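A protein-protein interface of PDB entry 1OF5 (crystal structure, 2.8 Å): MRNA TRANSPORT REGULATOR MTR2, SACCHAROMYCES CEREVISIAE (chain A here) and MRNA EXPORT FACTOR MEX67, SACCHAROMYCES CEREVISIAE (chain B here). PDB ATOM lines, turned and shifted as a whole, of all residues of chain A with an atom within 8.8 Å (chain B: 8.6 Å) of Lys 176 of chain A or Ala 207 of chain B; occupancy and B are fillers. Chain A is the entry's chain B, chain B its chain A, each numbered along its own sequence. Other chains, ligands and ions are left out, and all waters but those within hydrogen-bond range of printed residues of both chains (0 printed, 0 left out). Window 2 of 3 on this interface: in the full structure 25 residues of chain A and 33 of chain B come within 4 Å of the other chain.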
ATOM      1  N   ASN A  55      -3.541   6.266 -19.741  1.00  0.00           N
ATOM      2  CA  ASN A  55      -3.733   5.469 -18.505  1.00  0.00           C
ATOM      3  C   ASN A  55      -3.145   6.128 -17.226  1.00  0.00           C
ATOM      4  O   ASN A  55      -2.793   5.454 -16.246  1.00  0.00           O
ATOM      5  CB  ASN A  55      -3.211   4.069 -18.733  1.00  0.00           C
ATOM      6  CG  ASN A  55      -4.254   3.300 -19.518  1.00  0.00           C
ATOM      7  OD1 ASN A  55      -5.410   3.732 -19.627  1.00  0.00           O
ATOM      8  ND2 ASN A  55      -3.866   2.159 -20.082  1.00  0.00           N
ATOM      9  N   VAL A 102     -12.292  -2.584 -25.858  1.00  0.00           N
ATOM     10  CA  VAL A 102     -11.093  -3.172 -26.432  1.00  0.00           C
ATOM     11  C   VAL A 102     -10.876  -4.593 -25.965  1.00  0.00           C
ATOM     12  O   VAL A 102     -11.286  -4.961 -24.859  1.00  0.00           O
ATOM     13  CB  VAL A 102      -9.804  -2.364 -26.065  1.00  0.00           C
ATOM     14  CG1 VAL A 102      -8.845  -2.372 -27.241  1.00  0.00           C
ATOM     15  CG2 VAL A 102     -10.144  -0.937 -25.672  1.00  0.00           C
ATOM     16  N   PHE A 104      -7.745  -7.858 -26.055  1.00  0.00           N
ATOM     17  CA  PHE A 104      -6.294  -8.000 -26.114  1.00  0.00           C
ATOM     18  C   PHE A 104      -5.669  -9.317 -26.631  1.00  0.00           C
ATOM     19  O   PHE A 104      -4.528  -9.299 -27.123  1.00  0.00           O
ATOM     20  CB  PHE A 104      -5.695  -7.658 -24.736  1.00  0.00           C
ATOM     21  CG  PHE A 104      -5.954  -6.238 -24.295  1.00  0.00           C
ATOM     22  CD1 PHE A 104      -7.208  -5.855 -23.813  1.00  0.00           C
ATOM     23  CD2 PHE A 104      -4.954  -5.272 -24.381  1.00  0.00           C
ATOM     24  CE1 PHE A 104      -7.458  -4.529 -23.427  1.00  0.00           C
ATOM     25  CE2 PHE A 104      -5.195  -3.953 -23.999  1.00  0.00           C
ATOM     26  CZ  PHE A 104      -6.449  -3.582 -23.523  1.00  0.00           C
ATOM     27  N   PRO A 143     -12.123 -10.539 -23.119  1.00  0.00           N
ATOM     28  CA  PRO A 143     -13.270  -9.675 -22.817  1.00  0.00           C
ATOM     29  C   PRO A 143     -13.104  -8.262 -23.407  1.00  0.00           C
ATOM     30  O   PRO A 143     -12.072  -7.945 -24.000  1.00  0.00           O
ATOM     31  CB  PRO A 143     -13.279  -9.645 -21.292  1.00  0.00           C
ATOM     32  CG  PRO A 143     -12.695 -10.952 -20.908  1.00  0.00           C
ATOM     33  CD  PRO A 143     -11.562 -11.116 -21.885  1.00  0.00           C
ATOM     34  N   TYR A 144     -14.120  -7.423 -23.235  1.00  0.00           N
ATOM     35  CA  TYR A 144     -14.098  -6.041 -23.720  1.00  0.00           C
ATOM     36  C   TYR A 144     -13.836  -5.073 -22.564  1.00  0.00           C
ATOM     37  O   TYR A 144     -14.374  -5.240 -21.462  1.00  0.00           O
ATOM     38  CB  TYR A 144     -15.439  -5.676 -24.352  1.00  0.00           C
ATOM     39  CG  TYR A 144     -15.550  -5.931 -25.837  1.00  0.00           C
ATOM     40  CD1 TYR A 144     -16.796  -6.168 -26.432  1.00  0.00           C
ATOM     41  CD2 TYR A 144     -14.427  -5.893 -26.658  1.00  0.00           C
ATOM     42  CE1 TYR A 144     -16.915  -6.363 -27.810  1.00  0.00           C
ATOM     43  CE2 TYR A 144     -14.541  -6.078 -28.032  1.00  0.00           C
ATOM     44  CZ  TYR A 144     -15.779  -6.315 -28.601  1.00  0.00           C
ATOM     45  OH  TYR A 144     -15.867  -6.507 -29.960  1.00  0.00           O
ATOM     46  N   PHE A 145     -13.004  -4.067 -22.810  1.00  0.00           N
ATOM     47  CA  PHE A 145     -12.709  -3.076 -21.784  1.00  0.00           C
ATOM     48  C   PHE A 145     -13.221  -1.727 -22.272  1.00  0.00           C
ATOM     49  O   PHE A 145     -13.356  -1.496 -23.470  1.00  0.00           O
ATOM     50  CB  PHE A 145     -11.201  -2.976 -21.533  1.00  0.00           C
ATOM     51  CG  PHE A 145     -10.590  -4.218 -20.957  1.00  0.00           C
ATOM     52  CD1 PHE A 145     -10.562  -5.400 -21.687  1.00  0.00           C
ATOM     53  CD2 PHE A 145     -10.012  -4.196 -19.691  1.00  0.00           C
ATOM     54  CE1 PHE A 145      -9.962  -6.545 -21.168  1.00  0.00           C
ATOM     55  CE2 PHE A 145      -9.410  -5.334 -19.157  1.00  0.00           C
ATOM     56  CZ  PHE A 145      -9.383  -6.512 -19.896  1.00  0.00           C
ATOM     57  N   GLY A 146     -13.500  -0.829 -21.340  1.00  0.00           N
ATOM     58  CA  GLY A 146     -13.980   0.480 -21.721  1.00  0.00           C
ATOM     59  C   GLY A 146     -12.876   1.515 -21.755  1.00  0.00           C
ATOM     60  O   GLY A 146     -12.110   1.655 -20.792  1.00  0.00           O
ATOM     61  N   ILE A 147     -12.798   2.237 -22.871  1.00  0.00           N
ATOM     62  CA  ILE A 147     -11.804   3.286 -23.057  1.00  0.00           C
ATOM     63  C   ILE A 147     -12.484   4.610 -23.354  1.00  0.00           C
ATOM     64  O   ILE A 147     -13.406   4.669 -24.168  1.00  0.00           O
ATOM     65  CB  ILE A 147     -10.848   2.974 -24.247  1.00  0.00           C
ATOM     66  CG1 ILE A 147      -9.616   2.240 -23.740  1.00  0.00           C
ATOM     67  CG2 ILE A 147     -10.413   4.270 -24.959  1.00  0.00           C
ATOM     68  CD1 ILE A 147      -9.940   0.966 -23.031  1.00  0.00           C
ATOM     69  N   ASN A 172      -7.712   6.910 -21.768  1.00  0.00           N
ATOM     70  CA  ASN A 172      -7.811   6.266 -20.456  1.00  0.00           C
ATOM     71  C   ASN A 172      -8.837   5.166 -20.363  1.00  0.00           C
ATOM     72  O   ASN A 172      -9.979   5.326 -20.802  1.00  0.00           O
ATOM     73  CB  ASN A 172      -8.129   7.289 -19.374  1.00  0.00           C
ATOM     74  CG  ASN A 172      -7.004   8.252 -19.160  1.00  0.00           C
ATOM     75  OD1 ASN A 172      -5.934   7.867 -18.685  1.00  0.00           O
ATOM     76  ND2 ASN A 172      -7.224   9.519 -19.526  1.00  0.00           N
ATOM     77  N   MET A 173      -8.432   4.050 -19.769  1.00  0.00           N
ATOM     78  CA  MET A 173      -9.338   2.936 -19.604  1.00  0.00           C
ATOM     79  C   MET A 173     -10.282   3.263 -18.444  1.00  0.00           C
ATOM     80  O   MET A 173      -9.839   3.498 -17.317  1.00  0.00           O
ATOM     81  CB  MET A 173      -8.554   1.666 -19.312  1.00  0.00           C
ATOM     82  CG  MET A 173      -9.441   0.469 -19.001  1.00  0.00           C
ATOM     83  SD  MET A 173      -8.478  -0.971 -18.506  1.00  0.00           S
ATOM     84  CE  MET A 173      -8.073  -1.648 -20.160  1.00  0.00           C
ATOM     85  N   VAL A 174     -11.581   3.286 -18.716  1.00  0.00           N
ATOM     86  CA  VAL A 174     -12.545   3.600 -17.678  1.00  0.00           C
ATOM     87  C   VAL A 174     -13.128   2.365 -17.006  1.00  0.00           C
ATOM     88  O   VAL A 174     -13.472   2.398 -15.816  1.00  0.00           O
ATOM     89  CB  VAL A 174     -13.680   4.467 -18.225  1.00  0.00           C
ATOM     90  CG1 VAL A 174     -13.193   5.881 -18.403  1.00  0.00           C
ATOM     91  CG2 VAL A 174     -14.161   3.915 -19.546  1.00  0.00           C
ATOM     92  N   TYR A 175     -13.243   1.271 -17.753  1.00  0.00           N
ATOM     93  CA  TYR A 175     -13.774   0.049 -17.160  1.00  0.00           C
ATOM     94  C   TYR A 175     -13.255  -1.239 -17.798  1.00  0.00           C
ATOM     95  O   TYR A 175     -12.705  -1.245 -18.907  1.00  0.00           O
ATOM     96  CB  TYR A 175     -15.316   0.061 -17.172  1.00  0.00           C
ATOM     97  CG  TYR A 175     -15.955  -0.130 -18.535  1.00  0.00           C
ATOM     98  CD1 TYR A 175     -16.023  -1.393 -19.133  1.00  0.00           C
ATOM     99  CD2 TYR A 175     -16.479   0.958 -19.237  1.00  0.00           C
ATOM    100  CE1 TYR A 175     -16.593  -1.562 -20.395  1.00  0.00           C
ATOM    101  CE2 TYR A 175     -17.048   0.798 -20.496  1.00  0.00           C
ATOM    102  CZ  TYR A 175     -17.100  -0.461 -21.072  1.00  0.00           C
ATOM    103  OH  TYR A 175     -17.631  -0.598 -22.335  1.00  0.00           O
ATOM    104  N   LYS A 176     -13.420  -2.328 -17.058  1.00  0.00           N
ATOM    105  CA  LYS A 176     -13.000  -3.635 -17.511  1.00  0.00           C
ATOM    106  C   LYS A 176     -14.063  -4.693 -17.204  1.00  0.00           C
ATOM    107  O   LYS A 176     -15.043  -4.413 -16.513  1.00  0.00           O
ATOM    108  CB  LYS A 176     -11.647  -3.996 -16.880  1.00  0.00           C
ATOM    109  CG  LYS A 176     -11.362  -3.444 -15.497  1.00  0.00           C
ATOM    110  CD  LYS A 176      -9.926  -3.819 -15.102  1.00  0.00           C
ATOM    111  CE  LYS A 176      -9.512  -3.261 -13.753  1.00  0.00           C
ATOM    112  NZ  LYS A 176     -10.421  -3.711 -12.662  1.00  0.00           N
ATOM    113  N   PRO A 177     -13.888  -5.917 -17.735  1.00  0.00           N
ATOM    114  CA  PRO A 177     -14.779  -7.078 -17.574  1.00  0.00           C
ATOM    115  C   PRO A 177     -15.449  -7.230 -16.198  1.00  0.00           C
ATOM    116  O   PRO A 177     -14.771  -7.496 -15.204  1.00  0.00           O
ATOM    117  CB  PRO A 177     -13.858  -8.247 -17.903  1.00  0.00           C
ATOM    118  CG  PRO A 177     -13.004  -7.665 -18.997  1.00  0.00           C
ATOM    119  CD  PRO A 177     -12.682  -6.287 -18.506  1.00  0.00           C
ATOM    120  N   GLU A 178     -16.775  -7.073 -16.168  1.00  0.00           N
ATOM    121  CA  GLU A 178     -17.583  -7.173 -14.946  1.00  0.00           C
ATOM    122  C   GLU A 178     -16.775  -6.863 -13.702  1.00  0.00           C
ATOM    123  O   GLU A 178     -16.427  -7.785 -12.955  1.00  0.00           O
ATOM    124  CB  GLU A 178     -18.179  -8.581 -14.792  1.00  0.00           C
ATOM    125  CG  GLU A 178     -18.386  -9.334 -16.104  1.00  0.00           C
ATOM    126  CD  GLU A 178     -19.581  -8.840 -16.904  1.00  0.00           C
ATOM    127  OE1 GLU A 178     -20.713  -9.304 -16.627  1.00  0.00           O
ATOM    128  OE2 GLU A 178     -19.384  -7.997 -17.811  1.00  0.00           O
ATOM    129  N   ASN B 113     -12.213   8.512  -4.468  1.00  0.00           N
ATOM    130  CA  ASN B 113     -11.640   7.350  -5.134  1.00  0.00           C
ATOM    131  C   ASN B 113     -12.468   6.802  -6.303  1.00  0.00           C
ATOM    132  O   ASN B 113     -11.958   6.069  -7.162  1.00  0.00           O
ATOM    133  CB  ASN B 113     -11.446   6.264  -4.080  1.00  0.00           C
ATOM    134  CG  ASN B 113     -12.593   6.222  -3.091  1.00  0.00           C
ATOM    135  OD1 ASN B 113     -13.672   5.698  -3.386  1.00  0.00           O
ATOM    136  ND2 ASN B 113     -12.379   6.805  -1.914  1.00  0.00           N
ATOM    137  N   GLU B 114     -13.744   7.159  -6.330  1.00  0.00           N
ATOM    138  CA  GLU B 114     -14.642   6.688  -7.372  1.00  0.00           C
ATOM    139  C   GLU B 114     -14.608   7.544  -8.656  1.00  0.00           C
ATOM    140  O   GLU B 114     -15.492   7.432  -9.529  1.00  0.00           O
ATOM    141  CB  GLU B 114     -16.065   6.655  -6.815  1.00  0.00           C
ATOM    142  CG  GLU B 114     -16.779   5.353  -7.076  1.00  0.00           C
ATOM    143  CD  GLU B 114     -16.286   4.249  -6.173  1.00  0.00           C
ATOM    144  OE1 GLU B 114     -16.124   3.117  -6.677  1.00  0.00           O
ATOM    145  OE2 GLU B 114     -16.070   4.514  -4.966  1.00  0.00           O
ATOM    146  N   SER B 116     -11.756   9.635 -11.639  1.00  0.00           N
ATOM    147  CA  SER B 116     -10.399   9.885 -12.118  1.00  0.00           C
ATOM    148  C   SER B 116     -10.413  11.193 -12.928  1.00  0.00           C
ATOM    149  O   SER B 116     -11.448  11.593 -13.456  1.00  0.00           O
ATOM    150  CB  SER B 116      -9.871   8.703 -12.941  1.00  0.00           C
ATOM    151  OG  SER B 116     -10.588   8.518 -14.138  1.00  0.00           O
ATOM    152  N   HIS B 133     -13.902  11.343 -14.996  1.00  0.00           N
ATOM    153  CA  HIS B 133     -14.499  10.021 -15.145  1.00  0.00           C
ATOM    154  C   HIS B 133     -15.059   9.603 -13.778  1.00  0.00           C
ATOM    155  O   HIS B 133     -14.421   9.837 -12.740  1.00  0.00           O
ATOM    156  CB  HIS B 133     -13.429   9.022 -15.587  1.00  0.00           C
ATOM    157  CG  HIS B 133     -12.639   9.472 -16.777  1.00  0.00           C
ATOM    158  ND1 HIS B 133     -13.116   9.381 -18.070  1.00  0.00           N
ATOM    159  CD2 HIS B 133     -11.410  10.034 -16.871  1.00  0.00           C
ATOM    160  CE1 HIS B 133     -12.214   9.864 -18.908  1.00  0.00           C
ATOM    161  NE2 HIS B 133     -11.169  10.267 -18.206  1.00  0.00           N
ATOM    162  N   SER B 177     -22.462   5.557 -14.804  1.00  0.00           N
ATOM    163  CA  SER B 177     -21.089   6.012 -15.022  1.00  0.00           C
ATOM    164  C   SER B 177     -21.098   7.096 -16.088  1.00  0.00           C
ATOM    165  O   SER B 177     -22.078   7.258 -16.814  1.00  0.00           O
ATOM    166  CB  SER B 177     -20.193   4.855 -15.457  1.00  0.00           C
ATOM    167  OG  SER B 177     -19.919   4.016 -14.347  1.00  0.00           O
ATOM    168  N   ARG B 201     -23.037   6.630 -19.477  1.00  0.00           N
ATOM    169  CA  ARG B 201     -22.930   5.213 -19.801  1.00  0.00           C
ATOM    170  C   ARG B 201     -23.312   4.300 -18.638  1.00  0.00           C
ATOM    171  O   ARG B 201     -23.462   4.747 -17.497  1.00  0.00           O
ATOM    172  CB  ARG B 201     -21.500   4.875 -20.286  1.00  0.00           C
ATOM    173  CG  ARG B 201     -20.426   4.891 -19.203  1.00  0.00           C
ATOM    174  CD  ARG B 201     -19.064   4.408 -19.731  1.00  0.00           C
ATOM    175  NE  ARG B 201     -18.129   4.128 -18.638  1.00  0.00           N
ATOM    176  CZ  ARG B 201     -17.347   5.036 -18.056  1.00  0.00           C
ATOM    177  NH1 ARG B 201     -17.369   6.297 -18.469  1.00  0.00           N
ATOM    178  NH2 ARG B 201     -16.569   4.689 -17.031  1.00  0.00           N
ATOM    179  N   TYR B 203     -23.470   2.103 -15.588  1.00  0.00           N
ATOM    180  CA  TYR B 203     -22.635   2.149 -14.408  1.00  0.00           C
ATOM    181  C   TYR B 203     -21.729   0.937 -14.315  1.00  0.00           C
ATOM    182  O   TYR B 203     -22.130  -0.185 -14.627  1.00  0.00           O
ATOM    183  CB  TYR B 203     -23.456   2.207 -13.132  1.00  0.00           C
ATOM    184  CG  TYR B 203     -22.559   2.117 -11.927  1.00  0.00           C
ATOM    185  CD1 TYR B 203     -21.833   3.230 -11.493  1.00  0.00           C
ATOM    186  CD2 TYR B 203     -22.364   0.908 -11.269  1.00  0.00           C
ATOM    187  CE1 TYR B 203     -20.931   3.139 -10.435  1.00  0.00           C
ATOM    188  CE2 TYR B 203     -21.473   0.802 -10.212  1.00  0.00           C
ATOM    189  CZ  TYR B 203     -20.756   1.918  -9.797  1.00  0.00           C
ATOM    190  OH  TYR B 203     -19.860   1.802  -8.753  1.00  0.00           O
ATOM    191  N   SER B 204     -20.504   1.179 -13.867  1.00  0.00           N
ATOM    192  CA  SER B 204     -19.508   0.134 -13.681  1.00  0.00           C
ATOM    193  C   SER B 204     -18.381   0.716 -12.836  1.00  0.00           C
ATOM    194  O   SER B 204     -18.170   1.925 -12.811  1.00  0.00           O
ATOM    195  CB  SER B 204     -18.970  -0.350 -15.028  1.00  0.00           C
ATOM    196  OG  SER B 204     -18.552   0.749 -15.803  1.00  0.00           O
ATOM    197  N   THR B 205     -17.671  -0.151 -12.129  1.00  0.00           N
ATOM    198  CA  THR B 205     -16.572   0.276 -11.280  1.00  0.00           C
ATOM    199  C   THR B 205     -15.399   0.817 -12.094  1.00  0.00           C
ATOM    200  O   THR B 205     -14.965   0.203 -13.071  1.00  0.00           O
ATOM    201  CB  THR B 205     -16.111  -0.897 -10.401  1.00  0.00           C
ATOM    202  OG1 THR B 205     -17.197  -1.296  -9.547  1.00  0.00           O
ATOM    203  CG2 THR B 205     -14.923  -0.496  -9.553  1.00  0.00           C
ATOM    204  N   GLY B 206     -14.892   1.973 -11.684  1.00  0.00           N
ATOM    205  CA  GLY B 206     -13.778   2.587 -12.389  1.00  0.00           C
ATOM    206  C   GLY B 206     -12.522   1.733 -12.424  1.00  0.00           C
ATOM    207  O   GLY B 206     -11.931   1.431 -11.382  1.00  0.00           O
ATOM    208  N   ALA B 207     -12.107   1.350 -13.628  1.00  0.00           N
ATOM    209  CA  ALA B 207     -10.918   0.519 -13.805  1.00  0.00           C
ATOM    210  C   ALA B 207      -9.658   1.233 -13.337  1.00  0.00           C
ATOM    211  O   ALA B 207      -8.551   0.756 -13.575  1.00  0.00           O
ATOM    212  CB  ALA B 207     -10.766   0.134 -15.277  1.00  0.00           C
ATOM    213  N   TRP B 208      -9.827   2.361 -12.654  1.00  0.00           N
ATOM    214  CA  TRP B 208      -8.690   3.151 -12.199  1.00  0.00           C
ATOM    215  C   TRP B 208      -8.386   3.128 -10.697  1.00  0.00           C
ATOM    216  O   TRP B 208      -7.271   3.450 -10.279  1.00  0.00           O
ATOM    217  CB  TRP B 208      -8.898   4.601 -12.643  1.00  0.00           C
ATOM    218  CG  TRP B 208     -10.153   5.220 -12.083  1.00  0.00           C
ATOM    219  CD1 TRP B 208     -10.370   5.613 -10.789  1.00  0.00           C
ATOM    220  CD2 TRP B 208     -11.376   5.480 -12.792  1.00  0.00           C
ATOM    221  NE1 TRP B 208     -11.650   6.108 -10.652  1.00  0.00           N
ATOM    222  CE2 TRP B 208     -12.285   6.048 -11.865  1.00  0.00           C
ATOM    223  CE3 TRP B 208     -11.782   5.317 -14.122  1.00  0.00           C
ATOM    224  CZ2 TRP B 208     -13.584   6.418 -12.219  1.00  0.00           C
ATOM    225  CZ3 TRP B 208     -13.081   5.691 -14.477  1.00  0.00           C
ATOM    226  CH2 TRP B 208     -13.958   6.246 -13.530  1.00  0.00           C
ATOM    227  N   LYS B 209      -9.369   2.749  -9.890  1.00  0.00           N
ATOM    228  CA  LYS B 209      -9.224   2.738  -8.435  1.00  0.00           C
ATOM    229  C   LYS B 209      -7.916   2.173  -7.861  1.00  0.00           C
ATOM    230  O   LYS B 209      -7.200   1.419  -8.515  1.00  0.00           O
ATOM    231  CB  LYS B 209     -10.403   1.994  -7.810  1.00  0.00           C
ATOM    232  CG  LYS B 209     -11.739   2.284  -8.457  1.00  0.00           C
ATOM    233  CD  LYS B 209     -12.843   1.504  -7.771  1.00  0.00           C
ATOM    234  CE  LYS B 209     -12.450   0.027  -7.566  1.00  0.00           C
ATOM    235  NZ  LYS B 209     -11.992  -0.707  -8.796  1.00  0.00           N
ATOM    236  N   THR B 210      -7.614   2.574  -6.628  1.00  0.00           N
ATOM    237  CA  THR B 210      -6.427   2.114  -5.909  1.00  0.00           C
ATOM    238  C   THR B 210      -6.773   2.159  -4.419  1.00  0.00           C
ATOM    239  O   THR B 210      -7.916   2.468  -4.054  1.00  0.00           O
ATOM    240  CB  THR B 210      -5.165   3.013  -6.177  1.00  0.00           C
ATOM    241  OG1 THR B 210      -5.318   4.284  -5.534  1.00  0.00           O
ATOM    242  CG2 THR B 210      -4.975   3.240  -7.660  1.00  0.00           C
ATOM    243  N   ALA B 216      -8.010  10.148  -8.801  1.00  0.00           N
ATOM    244  CA  ALA B 216      -6.825   9.741  -9.551  1.00  0.00           C
ATOM    245  C   ALA B 216      -6.567  10.889 -10.529  1.00  0.00           C
ATOM    246  O   ALA B 216      -7.331  11.086 -11.480  1.00  0.00           O
ATOM    247  CB  ALA B 216      -7.093   8.457 -10.307  1.00  0.00           C
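The backbone NH (N) of Ala 207 of chain B is in hydrogen-bond range of the backbone carbonyl oxygen (O) of Val 174 of chain A (2.8 Å).
The backbone NH of Arg 201 of chain B lies within hydrogen-bond range of the backbone carbonyl oxygen of Ser 177 of chain B (2.9 Å). OG of Ser 177 of chain B lies within hydrogen-bond range of N of Ser 204 of chain B (2.9 Å). The side-chain amino group (NZ) of Lys 209 of chain B lies close to the backbone carbonyl oxygen (O) of Gly 206 of chain B, at 3.4 Å. The side-chain amide oxygen (OD1) of Asn 55 of chain A is in hydrogen-bond range of the backbone NH (N) of Met 173 of chain A (3.0 Å). N of Val 174 of chain A is in hydrogen-bond range of O of Gly 146 of chain A (2.7 Å). The backbone NH of Gly 146 of chain A is in hydrogen-bond range of the backbone carbonyl oxygen of Tyr 175 of chain A.
Among the printed residues, pairs that only touch across the chains: Val 174 of chain A with Arg 201 of chain B, Val 174 of chain A with Gly 206 of chain B, Val 174 of chain A with His 133 of chain B, Tyr 175 of chain A with Ala 207 of chain B, Val 174 of chain A with Trp 208 of chain B, Tyr 175 of chain A with Ser 204 of chain B, Tyr 175 of chain A with Arg 201 of chain B, Lys 176 of chain A with Ala 207 of chain B, Val 174 of chain A with Thr 205 of chain B and Met 173 of chain A with Ala 207 of chain B.
Of the printed residues of chain B, Met 173 of chain A touches Ala 207 (3.97 Å). Of the printed residues of chain B, Val 174 of chain A touches His 133 (3.5 Å), Arg 201 (3.1 Å), Thr 205 (3.8 Å), Gly 206 (3.4 Å), Ala 207 (2.8 Å) and Trp 208 (3.6 Å). No residue of chain B comes within 4 Å of Pro 177 of chain A. Ser 177 of chain B touches none of the printed residues of chain A. Of the printed residues of chain A, Arg 201 of chain B touches Val 174 (3.1 Å) and Tyr 175 (3.6 Å). Of the printed residues of chain A, Ser 204 of chain B touches Tyr 175 (3.6 Å). Gly 206 of chain B touches one residue of chain A. Of chain A, only Met 173, Val 174, Tyr 175 and Lys 176 come within 4 Å of Ala 207 of chain B. Thr 210 of chain B touches none of the printed residues of chain A. The nearest residue of chain B that does not touch Lys 176 of chain A is Thr 205 of chain B (5.0 Å). The nearest residue of chain A that does not touch Ala 207 of chain B is Gly 146 of chain A (5.9 Å).
Of the 15 printed residues of chain A, 4 touch a printed residue of chain B. Hydrophobic or aromatic side chains of chain A that line the printed part of chain B: Met 173, Val 174 and Tyr 175. Among the printed residues, no Asp or Glu carboxylate lies within 4 Å of a Lys or Arg side-chain nitrogen of the other chain.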
